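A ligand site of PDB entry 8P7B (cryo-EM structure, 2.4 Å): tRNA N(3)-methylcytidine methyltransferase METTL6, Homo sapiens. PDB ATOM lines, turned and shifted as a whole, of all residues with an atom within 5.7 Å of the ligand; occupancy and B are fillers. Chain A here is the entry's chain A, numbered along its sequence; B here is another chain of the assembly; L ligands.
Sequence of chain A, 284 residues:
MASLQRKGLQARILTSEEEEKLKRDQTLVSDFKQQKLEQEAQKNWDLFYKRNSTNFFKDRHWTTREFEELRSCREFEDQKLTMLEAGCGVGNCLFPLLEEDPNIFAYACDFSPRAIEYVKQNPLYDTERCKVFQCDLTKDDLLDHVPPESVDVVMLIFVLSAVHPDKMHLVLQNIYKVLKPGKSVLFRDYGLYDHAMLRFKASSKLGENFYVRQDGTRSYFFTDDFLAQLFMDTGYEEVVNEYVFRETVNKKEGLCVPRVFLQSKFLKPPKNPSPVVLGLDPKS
The side-chain hydroxyl (OH) of Tyr 49 sits at hydrogen-bond distance from an oxygen (O4) of the ligand (2.4 Å). O of Ile 157 sits at hydrogen-bond distance from N1 of the ligand, at 2.5 Å. The guanidinium group (NH1) of Arg 60 lies within salt-bridge range of an oxygen (O2) of the ligand, 2.5 Å away. A nitrogen (N5) of the ligand sits at hydrogen-bond distance from the backbone NH (N) of Leu 137 (3.0 Å). OD1 of Asp 110 is in hydrogen-bond range of O5 of the ligand. O of Gly 87 lies close to N1 of the ligand, at 3.2 Å.
An oxygen (O1) of the ligand sits close to the backbone carbonyl oxygen (O) of Gly 91, at 3.3 Å. CE3 of Trp 45 touches C7 of the ligand (3.7 Å). Gly 89 touches the ligand (CA to O4, 3.8 Å). Asn 92 touches the ligand (CB to O1, 3.6 Å). Cys 93 touches the ligand. Phe 111 touches the ligand. Cys 135 touches the ligand (O to C13, 3.4 Å). OD1 of Asp 136 touches N4 of the ligand, at 3.8 Å. Thr 138 touches the ligand (CG2 to N4, 3.9 Å). O of Phe 158 touches C5 of the ligand (3.6 Å). Val 159 touches the ligand (CG2 to N1, 3.3 Å). Ala 162 touches the ligand (CB to C10, 3.8 Å). Val 163 touches the ligand (CG2 to N4, 3.7 Å). JMH 32 of chain B touches the ligand. Hydrophobic or aromatic side chains within 4 Å of the ligand: Trp 45, Tyr 49, Phe 111, Leu 137, Val 159, Ala 162 and Val 163.
O2' of JMH 32 of chain B sits close to the guanidinium group (NH2) of Arg 60 (3.3 Å). N of Arg 60 is in hydrogen-bond range of O of Asn 92. O of Asp 110 lies within hydrogen-bond range of N of Cys 135 (3.2 Å). The backbone NH (N) of Gly 89 sits at hydrogen-bond distance from the side-chain carboxylate (OD2) of Asp 110. OD1 of Asp 110 sits at hydrogen-bond distance from N of Ser 112, at 2.6 Å. The backbone NH of Gly 87 is in hydrogen-bond range of the backbone carbonyl oxygen of Cys 109 (2.7 Å). SG of Cys 93 is in hydrogen-bond range of OE2 of Glu 85. OD1 of Asp 136 sits at hydrogen-bond distance from OG1 of Thr 138 (3.0 Å).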
ATOM      1  N   TRP A  45      -4.347  -0.627 -24.680  1.00  0.00           N
ATOM      2  CA  TRP A  45      -5.646  -0.635 -25.384  1.00  0.00           C
ATOM      3  C   TRP A  45      -5.485  -1.015 -26.851  1.00  0.00           C
ATOM      4  O   TRP A  45      -6.357  -1.682 -27.377  1.00  0.00           O
ATOM      5  CB  TRP A  45      -6.336   0.689 -25.170  1.00  0.00           C
ATOM      6  CG  TRP A  45      -7.080   0.717 -23.889  1.00  0.00           C
ATOM      7  CD1 TRP A  45      -6.822   1.516 -22.820  1.00  0.00           C
ATOM      8  CD2 TRP A  45      -8.279  -0.002 -23.593  1.00  0.00           C
ATOM      9  NE1 TRP A  45      -7.759   1.296 -21.850  1.00  0.00           N
ATOM     10  CE2 TRP A  45      -8.668   0.380 -22.295  1.00  0.00           C
ATOM     11  CE3 TRP A  45      -9.048  -0.944 -24.281  1.00  0.00           C
ATOM     12  CZ2 TRP A  45      -9.792  -0.151 -21.670  1.00  0.00           C
ATOM     13  CZ3 TRP A  45     -10.155  -1.467 -23.669  1.00  0.00           C
ATOM     14  CH2 TRP A  45     -10.513  -1.076 -22.380  1.00  0.00           C
ATOM     15  N   TYR A  49      -7.300  -4.374 -28.923  1.00  0.00           N
ATOM     16  CA  TYR A  49      -8.030  -4.425 -30.210  1.00  0.00           C
ATOM     17  C   TYR A  49      -7.289  -5.311 -31.195  1.00  0.00           C
ATOM     18  O   TYR A  49      -7.866  -5.612 -32.218  1.00  0.00           O
ATOM     19  CB  TYR A  49      -8.314  -3.025 -30.736  1.00  0.00           C
ATOM     20  CG  TYR A  49      -9.310  -2.290 -29.918  1.00  0.00           C
ATOM     21  CD1 TYR A  49     -10.601  -2.758 -29.785  1.00  0.00           C
ATOM     22  CD2 TYR A  49      -8.954  -1.158 -29.220  1.00  0.00           C
ATOM     23  CE1 TYR A  49     -11.537  -2.094 -29.022  1.00  0.00           C
ATOM     24  CE2 TYR A  49      -9.865  -0.486 -28.434  1.00  0.00           C
ATOM     25  CZ  TYR A  49     -11.162  -0.958 -28.345  1.00  0.00           C
ATOM     26  OH  TYR A  49     -12.071  -0.307 -27.570  1.00  0.00           O
ATOM     27  N   PHE A  57     -16.461  -6.786 -26.982  1.00  0.00           N
ATOM     28  CA  PHE A  57     -17.623  -6.077 -26.397  1.00  0.00           C
ATOM     29  C   PHE A  57     -18.805  -6.240 -27.342  1.00  0.00           C
ATOM     30  O   PHE A  57     -18.605  -6.526 -28.519  1.00  0.00           O
ATOM     31  CB  PHE A  57     -17.283  -4.633 -26.070  1.00  0.00           C
ATOM     32  CG  PHE A  57     -16.213  -4.453 -25.029  1.00  0.00           C
ATOM     33  CD1 PHE A  57     -16.387  -4.956 -23.754  1.00  0.00           C
ATOM     34  CD2 PHE A  57     -15.028  -3.810 -25.325  1.00  0.00           C
ATOM     35  CE1 PHE A  57     -15.395  -4.801 -22.795  1.00  0.00           C
ATOM     36  CE2 PHE A  57     -14.042  -3.666 -24.374  1.00  0.00           C
ATOM     37  CZ  PHE A  57     -14.229  -4.156 -23.107  1.00  0.00           C
ATOM     38  N   ARG A  60     -24.402  -1.813 -27.451  1.00  0.00           N
ATOM     39  CA  ARG A  60     -25.216  -1.391 -26.298  1.00  0.00           C
ATOM     40  C   ARG A  60     -26.532  -0.835 -26.842  1.00  0.00           C
ATOM     41  O   ARG A  60     -26.517   0.269 -27.392  1.00  0.00           O
ATOM     42  CB  ARG A  60     -24.460  -0.350 -25.469  1.00  0.00           C
ATOM     43  CG  ARG A  60     -23.165  -0.889 -24.892  1.00  0.00           C
ATOM     44  CD  ARG A  60     -22.322   0.162 -24.176  1.00  0.00           C
ATOM     45  NE  ARG A  60     -21.147  -0.473 -23.609  1.00  0.00           N
ATOM     46  CZ  ARG A  60     -20.106  -0.872 -24.323  1.00  0.00           C
ATOM     47  NH1 ARG A  60     -20.085  -0.681 -25.622  1.00  0.00           N
ATOM     48  NH2 ARG A  60     -19.079  -1.452 -23.733  1.00  0.00           N
ATOM     49  N   GLU A  85     -18.587  11.239 -28.963  1.00  0.00           N
ATOM     50  CA  GLU A  85     -18.435   9.960 -28.272  1.00  0.00           C
ATOM     51  C   GLU A  85     -16.980   9.816 -27.859  1.00  0.00           C
ATOM     52  O   GLU A  85     -16.147   9.375 -28.650  1.00  0.00           O
ATOM     53  CB  GLU A  85     -18.885   8.809 -29.160  1.00  0.00           C
ATOM     54  CG  GLU A  85     -18.788   7.465 -28.482  1.00  0.00           C
ATOM     55  CD  GLU A  85     -19.724   7.350 -27.292  1.00  0.00           C
ATOM     56  OE1 GLU A  85     -20.772   8.016 -27.308  1.00  0.00           O
ATOM     57  OE2 GLU A  85     -19.397   6.608 -26.346  1.00  0.00           O
ATOM     58  N   ALA A  86     -16.674  10.195 -26.621  1.00  0.00           N
ATOM     59  CA  ALA A  86     -15.317  10.101 -26.104  1.00  0.00           C
ATOM     60  C   ALA A  86     -15.013   8.644 -25.761  1.00  0.00           C
ATOM     61  O   ALA A  86     -15.746   8.020 -24.994  1.00  0.00           O
ATOM     62  CB  ALA A  86     -15.162  10.986 -24.871  1.00  0.00           C
ATOM     63  N   GLY A  87     -13.936   8.103 -26.321  1.00  0.00           N
ATOM     64  CA  GLY A  87     -13.664   6.702 -26.147  1.00  0.00           C
ATOM     65  C   GLY A  87     -14.679   5.874 -26.904  1.00  0.00           C
ATOM     66  O   GLY A  87     -15.516   5.200 -26.313  1.00  0.00           O
ATOM     67  N   CYS A  88     -14.630   5.944 -28.239  1.00  0.00           N
ATOM     68  CA  CYS A  88     -15.633   5.304 -29.063  1.00  0.00           C
ATOM     69  C   CYS A  88     -15.404   3.812 -29.237  1.00  0.00           C
ATOM     70  O   CYS A  88     -16.330   3.109 -29.665  1.00  0.00           O
ATOM     71  CB  CYS A  88     -15.692   5.978 -30.433  1.00  0.00           C
ATOM     72  SG  CYS A  88     -14.151   5.905 -31.361  1.00  0.00           S
ATOM     73  N   GLY A  89     -14.219   3.304 -28.912  1.00  0.00           N
ATOM     74  CA  GLY A  89     -13.969   1.902 -29.125  1.00  0.00           C
ATOM     75  C   GLY A  89     -14.045   1.550 -30.594  1.00  0.00           C
ATOM     76  O   GLY A  89     -13.575   2.303 -31.451  1.00  0.00           O
ATOM     77  N   VAL A  90     -14.636   0.396 -30.885  1.00  0.00           N
ATOM     78  CA  VAL A  90     -14.869  -0.025 -32.247  1.00  0.00           C
ATOM     79  C   VAL A  90     -16.314   0.244 -32.674  1.00  0.00           C
ATOM     80  O   VAL A  90     -16.826  -0.401 -33.584  1.00  0.00           O
ATOM     81  CB  VAL A  90     -14.496  -1.494 -32.461  1.00  0.00           C
ATOM     82  CG1 VAL A  90     -13.010  -1.691 -32.288  1.00  0.00           C
ATOM     83  CG2 VAL A  90     -15.270  -2.366 -31.513  1.00  0.00           C
ATOM     84  N   GLY A  91     -16.964   1.186 -32.017  1.00  0.00           N
ATOM     85  CA  GLY A  91     -18.395   1.354 -32.177  1.00  0.00           C
ATOM     86  C   GLY A  91     -19.086   0.924 -30.910  1.00  0.00           C
ATOM     87  O   GLY A  91     -18.771   1.424 -29.830  1.00  0.00           O
ATOM     88  N   ASN A  92     -20.074   0.030 -31.042  1.00  0.00           N
ATOM     89  CA  ASN A  92     -20.673  -0.672 -29.918  1.00  0.00           C
ATOM     90  C   ASN A  92     -21.419   0.268 -28.983  1.00  0.00           C
ATOM     91  O   ASN A  92     -22.110  -0.175 -28.060  1.00  0.00           O
ATOM     92  CB  ASN A  92     -19.605  -1.435 -29.127  1.00  0.00           C
ATOM     93  CG  ASN A  92     -19.170  -2.699 -29.826  1.00  0.00           C
ATOM     94  OD1 ASN A  92     -18.017  -3.119 -29.719  1.00  0.00           O
ATOM     95  ND2 ASN A  92     -20.081  -3.315 -30.565  1.00  0.00           N
ATOM     96  N   CYS A  93     -21.299   1.573 -29.205  1.00  0.00           N
ATOM     97  CA  CYS A  93     -22.049   2.552 -28.438  1.00  0.00           C
ATOM     98  C   CYS A  93     -22.661   3.656 -29.287  1.00  0.00           C
ATOM     99  O   CYS A  93     -23.676   4.227 -28.866  1.00  0.00           O
ATOM    100  CB  CYS A  93     -21.166   3.182 -27.360  1.00  0.00           C
ATOM    101  SG  CYS A  93     -21.906   4.561 -26.459  1.00  0.00           S
ATOM    102  N   CYS A 109     -14.001   9.828 -30.693  1.00  0.00           N
ATOM    103  CA  CYS A 109     -12.675  10.065 -30.130  1.00  0.00           C
ATOM    104  C   CYS A 109     -12.157   8.774 -29.511  1.00  0.00           C
ATOM    105  O   CYS A 109     -12.881   8.094 -28.795  1.00  0.00           O
ATOM    106  CB  CYS A 109     -12.754  11.164 -29.068  1.00  0.00           C
ATOM    107  SG  CYS A 109     -11.187  11.615 -28.339  1.00  0.00           S
ATOM    108  N   ASP A 110     -10.902   8.451 -29.828  1.00  0.00           N
ATOM    109  CA  ASP A 110     -10.243   7.244 -29.270  1.00  0.00           C
ATOM    110  C   ASP A 110      -8.729   7.397 -29.478  1.00  0.00           C
ATOM    111  O   ASP A 110      -8.335   7.797 -30.582  1.00  0.00           O
ATOM    112  CB  ASP A 110     -10.759   5.966 -29.926  1.00  0.00           C
ATOM    113  CG  ASP A 110     -10.322   4.727 -29.179  1.00  0.00           C
ATOM    114  OD1 ASP A 110      -9.103   4.486 -29.114  1.00  0.00           O
ATOM    115  OD2 ASP A 110     -11.188   4.046 -28.624  1.00  0.00           O
ATOM    116  N   PHE A 111      -7.934   7.063 -28.463  1.00  0.00           N
ATOM    117  CA  PHE A 111      -6.456   7.232 -28.595  1.00  0.00           C
ATOM    118  C   PHE A 111      -5.826   5.991 -29.223  1.00  0.00           C
ATOM    119  O   PHE A 111      -4.602   6.010 -29.453  1.00  0.00           O
ATOM    120  CB  PHE A 111      -5.816   7.706 -27.294  1.00  0.00           C
ATOM    121  CG  PHE A 111      -5.844   6.731 -26.143  1.00  0.00           C
ATOM    122  CD1 PHE A 111      -6.240   5.425 -26.323  1.00  0.00           C
ATOM    123  CD2 PHE A 111      -5.427   7.128 -24.881  1.00  0.00           C
ATOM    124  CE1 PHE A 111      -6.244   4.536 -25.266  1.00  0.00           C
ATOM    125  CE2 PHE A 111      -5.430   6.239 -23.825  1.00  0.00           C
ATOM    126  CZ  PHE A 111      -5.838   4.942 -24.022  1.00  0.00           C
ATOM    127  N   SER A 112      -6.611   4.955 -29.518  1.00  0.00           N
ATOM    128  CA  SER A 112      -6.045   3.730 -30.143  1.00  0.00           C
ATOM    129  C   SER A 112      -6.301   3.766 -31.655  1.00  0.00           C
ATOM    130  O   SER A 112      -7.466   3.827 -32.040  1.00  0.00           O
ATOM    131  CB  SER A 112      -6.621   2.490 -29.519  1.00  0.00           C
ATOM    132  OG  SER A 112      -6.390   1.366 -30.359  1.00  0.00           O
ATOM    133  N   ALA A 115      -8.713   0.908 -33.080  1.00  0.00           N
ATOM    134  CA  ALA A 115     -10.140   1.121 -32.878  1.00  0.00           C
ATOM    135  C   ALA A 115     -10.697   2.056 -33.939  1.00  0.00           C
ATOM    136  O   ALA A 115     -11.801   1.837 -34.457  1.00  0.00           O
ATOM    137  CB  ALA A 115     -10.388   1.692 -31.487  1.00  0.00           C
ATOM    138  N   CYS A 135      -7.672  10.970 -30.455  1.00  0.00           N
ATOM    139  CA  CYS A 135      -7.320  12.055 -29.542  1.00  0.00           C
ATOM    140  C   CYS A 135      -7.187  11.489 -28.144  1.00  0.00           C
ATOM    141  O   CYS A 135      -8.164  11.007 -27.572  1.00  0.00           O
ATOM    142  CB  CYS A 135      -8.379  13.151 -29.580  1.00  0.00           C
ATOM    143  SG  CYS A 135      -8.351  14.266 -28.167  1.00  0.00           S
ATOM    144  N   ASP A 136      -5.981  11.566 -27.593  1.00  0.00           N
ATOM    145  CA  ASP A 136      -5.752  11.216 -26.203  1.00  0.00           C
ATOM    146  C   ASP A 136      -6.401  12.280 -25.322  1.00  0.00           C
ATOM    147  O   ASP A 136      -5.910  13.404 -25.227  1.00  0.00           O
ATOM    148  CB  ASP A 136      -4.254  11.122 -25.942  1.00  0.00           C
ATOM    149  CG  ASP A 136      -3.918  10.524 -24.591  1.00  0.00           C
ATOM    150  OD1 ASP A 136      -4.696  10.727 -23.628  1.00  0.00           O
ATOM    151  OD2 ASP A 136      -2.872   9.855 -24.483  1.00  0.00           O
ATOM    152  N   LEU A 137      -7.510  11.925 -24.668  1.00  0.00           N
ATOM    153  CA  LEU A 137      -8.330  12.881 -23.947  1.00  0.00           C
ATOM    154  C   LEU A 137      -7.612  13.569 -22.794  1.00  0.00           C
ATOM    155  O   LEU A 137      -8.167  14.516 -22.222  1.00  0.00           O
ATOM    156  CB  LEU A 137      -9.579  12.204 -23.421  1.00  0.00           C
ATOM    157  CG  LEU A 137     -10.652  11.875 -24.445  1.00  0.00           C
ATOM    158  CD1 LEU A 137     -11.622  10.866 -23.873  1.00  0.00           C
ATOM    159  CD2 LEU A 137     -11.384  13.130 -24.849  1.00  0.00           C
ATOM    160  N   THR A 138      -6.421  13.126 -22.431  1.00  0.00           N
ATOM    161  CA  THR A 138      -5.646  13.794 -21.392  1.00  0.00           C
ATOM    162  C   THR A 138      -4.556  14.682 -21.950  1.00  0.00           C
ATOM    163  O   THR A 138      -4.374  15.803 -21.472  1.00  0.00           O
ATOM    164  CB  THR A 138      -5.014  12.753 -20.457  1.00  0.00           C
ATOM    165  OG1 THR A 138      -3.911  12.124 -21.115  1.00  0.00           O
ATOM    166  CG2 THR A 138      -6.026  11.710 -20.080  1.00  0.00           C
ATOM    167  N   ILE A 157     -19.163   6.286 -21.501  1.00  0.00           N
ATOM    168  CA  ILE A 157     -19.668   4.959 -21.182  1.00  0.00           C
ATOM    169  C   ILE A 157     -18.458   4.047 -21.026  1.00  0.00           C
ATOM    170  O   ILE A 157     -17.847   3.627 -22.015  1.00  0.00           O
ATOM    171  CB  ILE A 157     -20.622   4.444 -22.262  1.00  0.00           C
ATOM    172  CG1 ILE A 157     -21.750   5.438 -22.510  1.00  0.00           C
ATOM    173  CG2 ILE A 157     -21.186   3.101 -21.856  1.00  0.00           C
ATOM    174  CD1 ILE A 157     -22.411   5.942 -21.255  1.00  0.00           C
ATOM    175  N   PHE A 158     -18.111   3.741 -19.771  1.00  0.00           N
ATOM    176  CA  PHE A 158     -17.010   2.841 -19.461  1.00  0.00           C
ATOM    177  C   PHE A 158     -15.702   3.306 -20.109  1.00  0.00           C
ATOM    178  O   PHE A 158     -14.909   2.506 -20.606  1.00  0.00           O
ATOM    179  CB  PHE A 158     -17.344   1.403 -19.857  1.00  0.00           C
ATOM    180  CG  PHE A 158     -18.458   0.813 -19.055  1.00  0.00           C
ATOM    181  CD1 PHE A 158     -18.244   0.340 -17.778  1.00  0.00           C
ATOM    182  CD2 PHE A 158     -19.741   0.741 -19.578  1.00  0.00           C
ATOM    183  CE1 PHE A 158     -19.267  -0.201 -17.039  1.00  0.00           C
ATOM    184  CE2 PHE A 158     -20.770   0.206 -18.843  1.00  0.00           C
ATOM    185  CZ  PHE A 158     -20.534  -0.265 -17.574  1.00  0.00           C
ATOM    186  N   VAL A 159     -15.477   4.615 -20.087  1.00  0.00           N
ATOM    187  CA  VAL A 159     -14.281   5.207 -20.638  1.00  0.00           C
ATOM    188  C   VAL A 159     -13.421   5.834 -19.552  1.00  0.00           C
ATOM    189  O   VAL A 159     -12.186   5.761 -19.611  1.00  0.00           O
ATOM    190  CB  VAL A 159     -14.624   6.242 -21.730  1.00  0.00           C
ATOM    191  CG1 VAL A 159     -13.380   6.891 -22.266  1.00  0.00           C
ATOM    192  CG2 VAL A 159     -15.399   5.587 -22.843  1.00  0.00           C
ATOM    193  N   ALA A 162     -10.840   3.682 -17.422  1.00  0.00           N
ATOM    194  CA  ALA A 162      -9.560   3.331 -18.025  1.00  0.00           C
ATOM    195  C   ALA A 162      -8.534   4.444 -17.903  1.00  0.00           C
ATOM    196  O   ALA A 162      -7.391   4.257 -18.319  1.00  0.00           O
ATOM    197  CB  ALA A 162      -9.753   2.962 -19.484  1.00  0.00           C
ATOM    198  N   VAL A 163      -8.911   5.584 -17.358  1.00  0.00           N
ATOM    199  CA  VAL A 163      -8.038   6.732 -17.192  1.00  0.00           C
ATOM    200  C   VAL A 163      -7.520   6.755 -15.773  1.00  0.00           C
ATOM    201  O   VAL A 163      -8.236   6.360 -14.833  1.00  0.00           O
ATOM    202  CB  VAL A 163      -8.779   8.042 -17.546  1.00  0.00           C
ATOM    203  CG1 VAL A 163      -7.857   9.226 -17.444  1.00  0.00           C
ATOM    204  CG2 VAL A 163      -9.365   7.949 -18.944  1.00  0.00           C
ATOM    205  N   VAL A 171      -9.464  15.134 -18.544  1.00  0.00           N
ATOM    206  CA  VAL A 171     -10.462  14.786 -19.545  1.00  0.00           C
ATOM    207  C   VAL A 171     -11.711  15.643 -19.376  1.00  0.00           C
ATOM    208  O   VAL A 171     -12.304  16.108 -20.360  1.00  0.00           O
ATOM    209  CB  VAL A 171     -10.798  13.288 -19.472  1.00  0.00           C
ATOM    210  CG1 VAL A 171     -11.800  12.914 -20.529  1.00  0.00           C
ATOM    211  CG2 VAL A 171      -9.534  12.461 -19.641  1.00  0.00           C
ATOM    212  N1  JMH B  32     -17.610  -2.912 -20.514  1.00  0.00           N
ATOM    213  C2  JMH B  32     -16.965  -2.098 -21.311  1.00  0.00           C
ATOM    214  C5  JMH B  32     -15.631  -3.445 -19.483  1.00  0.00           C
ATOM    215  C1' JMH B  32     -19.032  -3.066 -20.605  1.00  0.00           C
ATOM    216  C2' JMH B  32     -19.414  -4.253 -20.862  1.00  0.00           C
ATOM    217  C3' JMH B  32     -20.815  -4.286 -20.297  1.00  0.00           C
ATOM    218  C4  JMH B  32     -14.999  -2.590 -20.360  1.00  0.00           C
ATOM    219  C4' JMH B  32     -20.586  -3.516 -18.994  1.00  0.00           C
ATOM    220  C5' JMH B  32     -20.393  -4.351 -17.756  1.00  0.00           C
ATOM    221  C6  JMH B  32     -16.991  -3.582 -19.593  1.00  0.00           C
ATOM    222  C31 JMH B  32     -14.964  -1.051 -22.125  1.00  0.00           C
ATOM    223  N3  JMH B  32     -15.682  -1.945 -21.246  1.00  0.00           N
ATOM    224  N4  JMH B  32     -13.577  -2.400 -20.309  1.00  0.00           N
ATOM    225  O2  JMH B  32     -17.554  -1.498 -22.123  1.00  0.00           O
ATOM    226  O2' JMH B  32     -19.453  -4.416 -22.338  1.00  0.00           O
ATOM    227  O3' JMH B  32     -21.741  -3.572 -21.115  1.00  0.00           O
ATOM    228  O4' JMH B  32     -19.515  -2.895 -19.108  1.00  0.00           O
ATOM    229  O5' JMH B  32     -20.167  -5.721 -18.070  1.00  0.00           O
ATOM    230  OP1 JMH B  32     -18.609  -5.766 -16.138  1.00  0.00           O
ATOM    231  OP2 JMH B  32     -19.541  -7.938 -17.101  1.00  0.00           O
ATOM    232  P   JMH B  32     -19.058  -6.555 -17.305  1.00  0.00           P
HETATM  233  N1  LIG L   1     -17.306   3.322 -24.396  1.00  0.00           N
HETATM  234  C1  LIG L   1     -17.059   2.590 -25.628  1.00  0.00           C
HETATM  235  C2  LIG L   1     -15.693   1.906 -25.577  1.00  0.00           C
HETATM  236  C3  LIG L   1     -15.304   1.393 -24.202  1.00  0.00           C
HETATM  237  S1  LIG L   1     -13.674   0.600 -24.217  1.00  0.00           S
HETATM  238  C4  LIG L   1     -18.146   1.574 -25.888  1.00  0.00           C
HETATM  239  O1  LIG L   1     -17.983   0.660 -26.709  1.00  0.00           O
HETATM  240  O2  LIG L   1     -19.216   1.633 -25.283  1.00  0.00           O
HETATM  241  C5  LIG L   1     -12.937   2.148 -23.629  1.00  0.00           C
HETATM  242  C6  LIG L   1     -12.215   2.861 -24.757  1.00  0.00           C
HETATM  243  O3  LIG L   1     -11.766   4.127 -24.322  1.00  0.00           O
HETATM  244  C7  LIG L   1     -10.980   2.102 -25.202  1.00  0.00           C
HETATM  245  O4  LIG L   1     -11.165   1.655 -26.509  1.00  0.00           O
HETATM  246  C8  LIG L   1      -9.848   3.095 -25.182  1.00  0.00           C
HETATM  247  O5  LIG L   1      -9.264   3.118 -26.450  1.00  0.00           O
HETATM  248  C9  LIG L   1     -10.520   4.415 -24.906  1.00  0.00           C
HETATM  249  N2  LIG L   1      -9.764   5.274 -23.999  1.00  0.00           N
HETATM  250  C10 LIG L   1      -9.316   4.958 -22.743  1.00  0.00           C
HETATM  251  N3  LIG L   1      -8.685   6.044 -22.241  1.00  0.00           N
HETATM  252  C11 LIG L   1      -8.747   7.033 -23.145  1.00  0.00           C
HETATM  253  C12 LIG L   1      -8.251   8.332 -23.146  1.00  0.00           C
HETATM  254  N4  LIG L   1      -7.600   8.801 -22.101  1.00  0.00           N
HETATM  255  N5  LIG L   1      -8.455   9.121 -24.250  1.00  0.00           N
HETATM  256  C13 LIG L   1      -9.142   8.635 -25.338  1.00  0.00           C
HETATM  257  N6  LIG L   1      -9.617   7.347 -25.327  1.00  0.00           N
HETATM  258  C14 LIG L   1      -9.408   6.557 -24.256  1.00  0.00           C
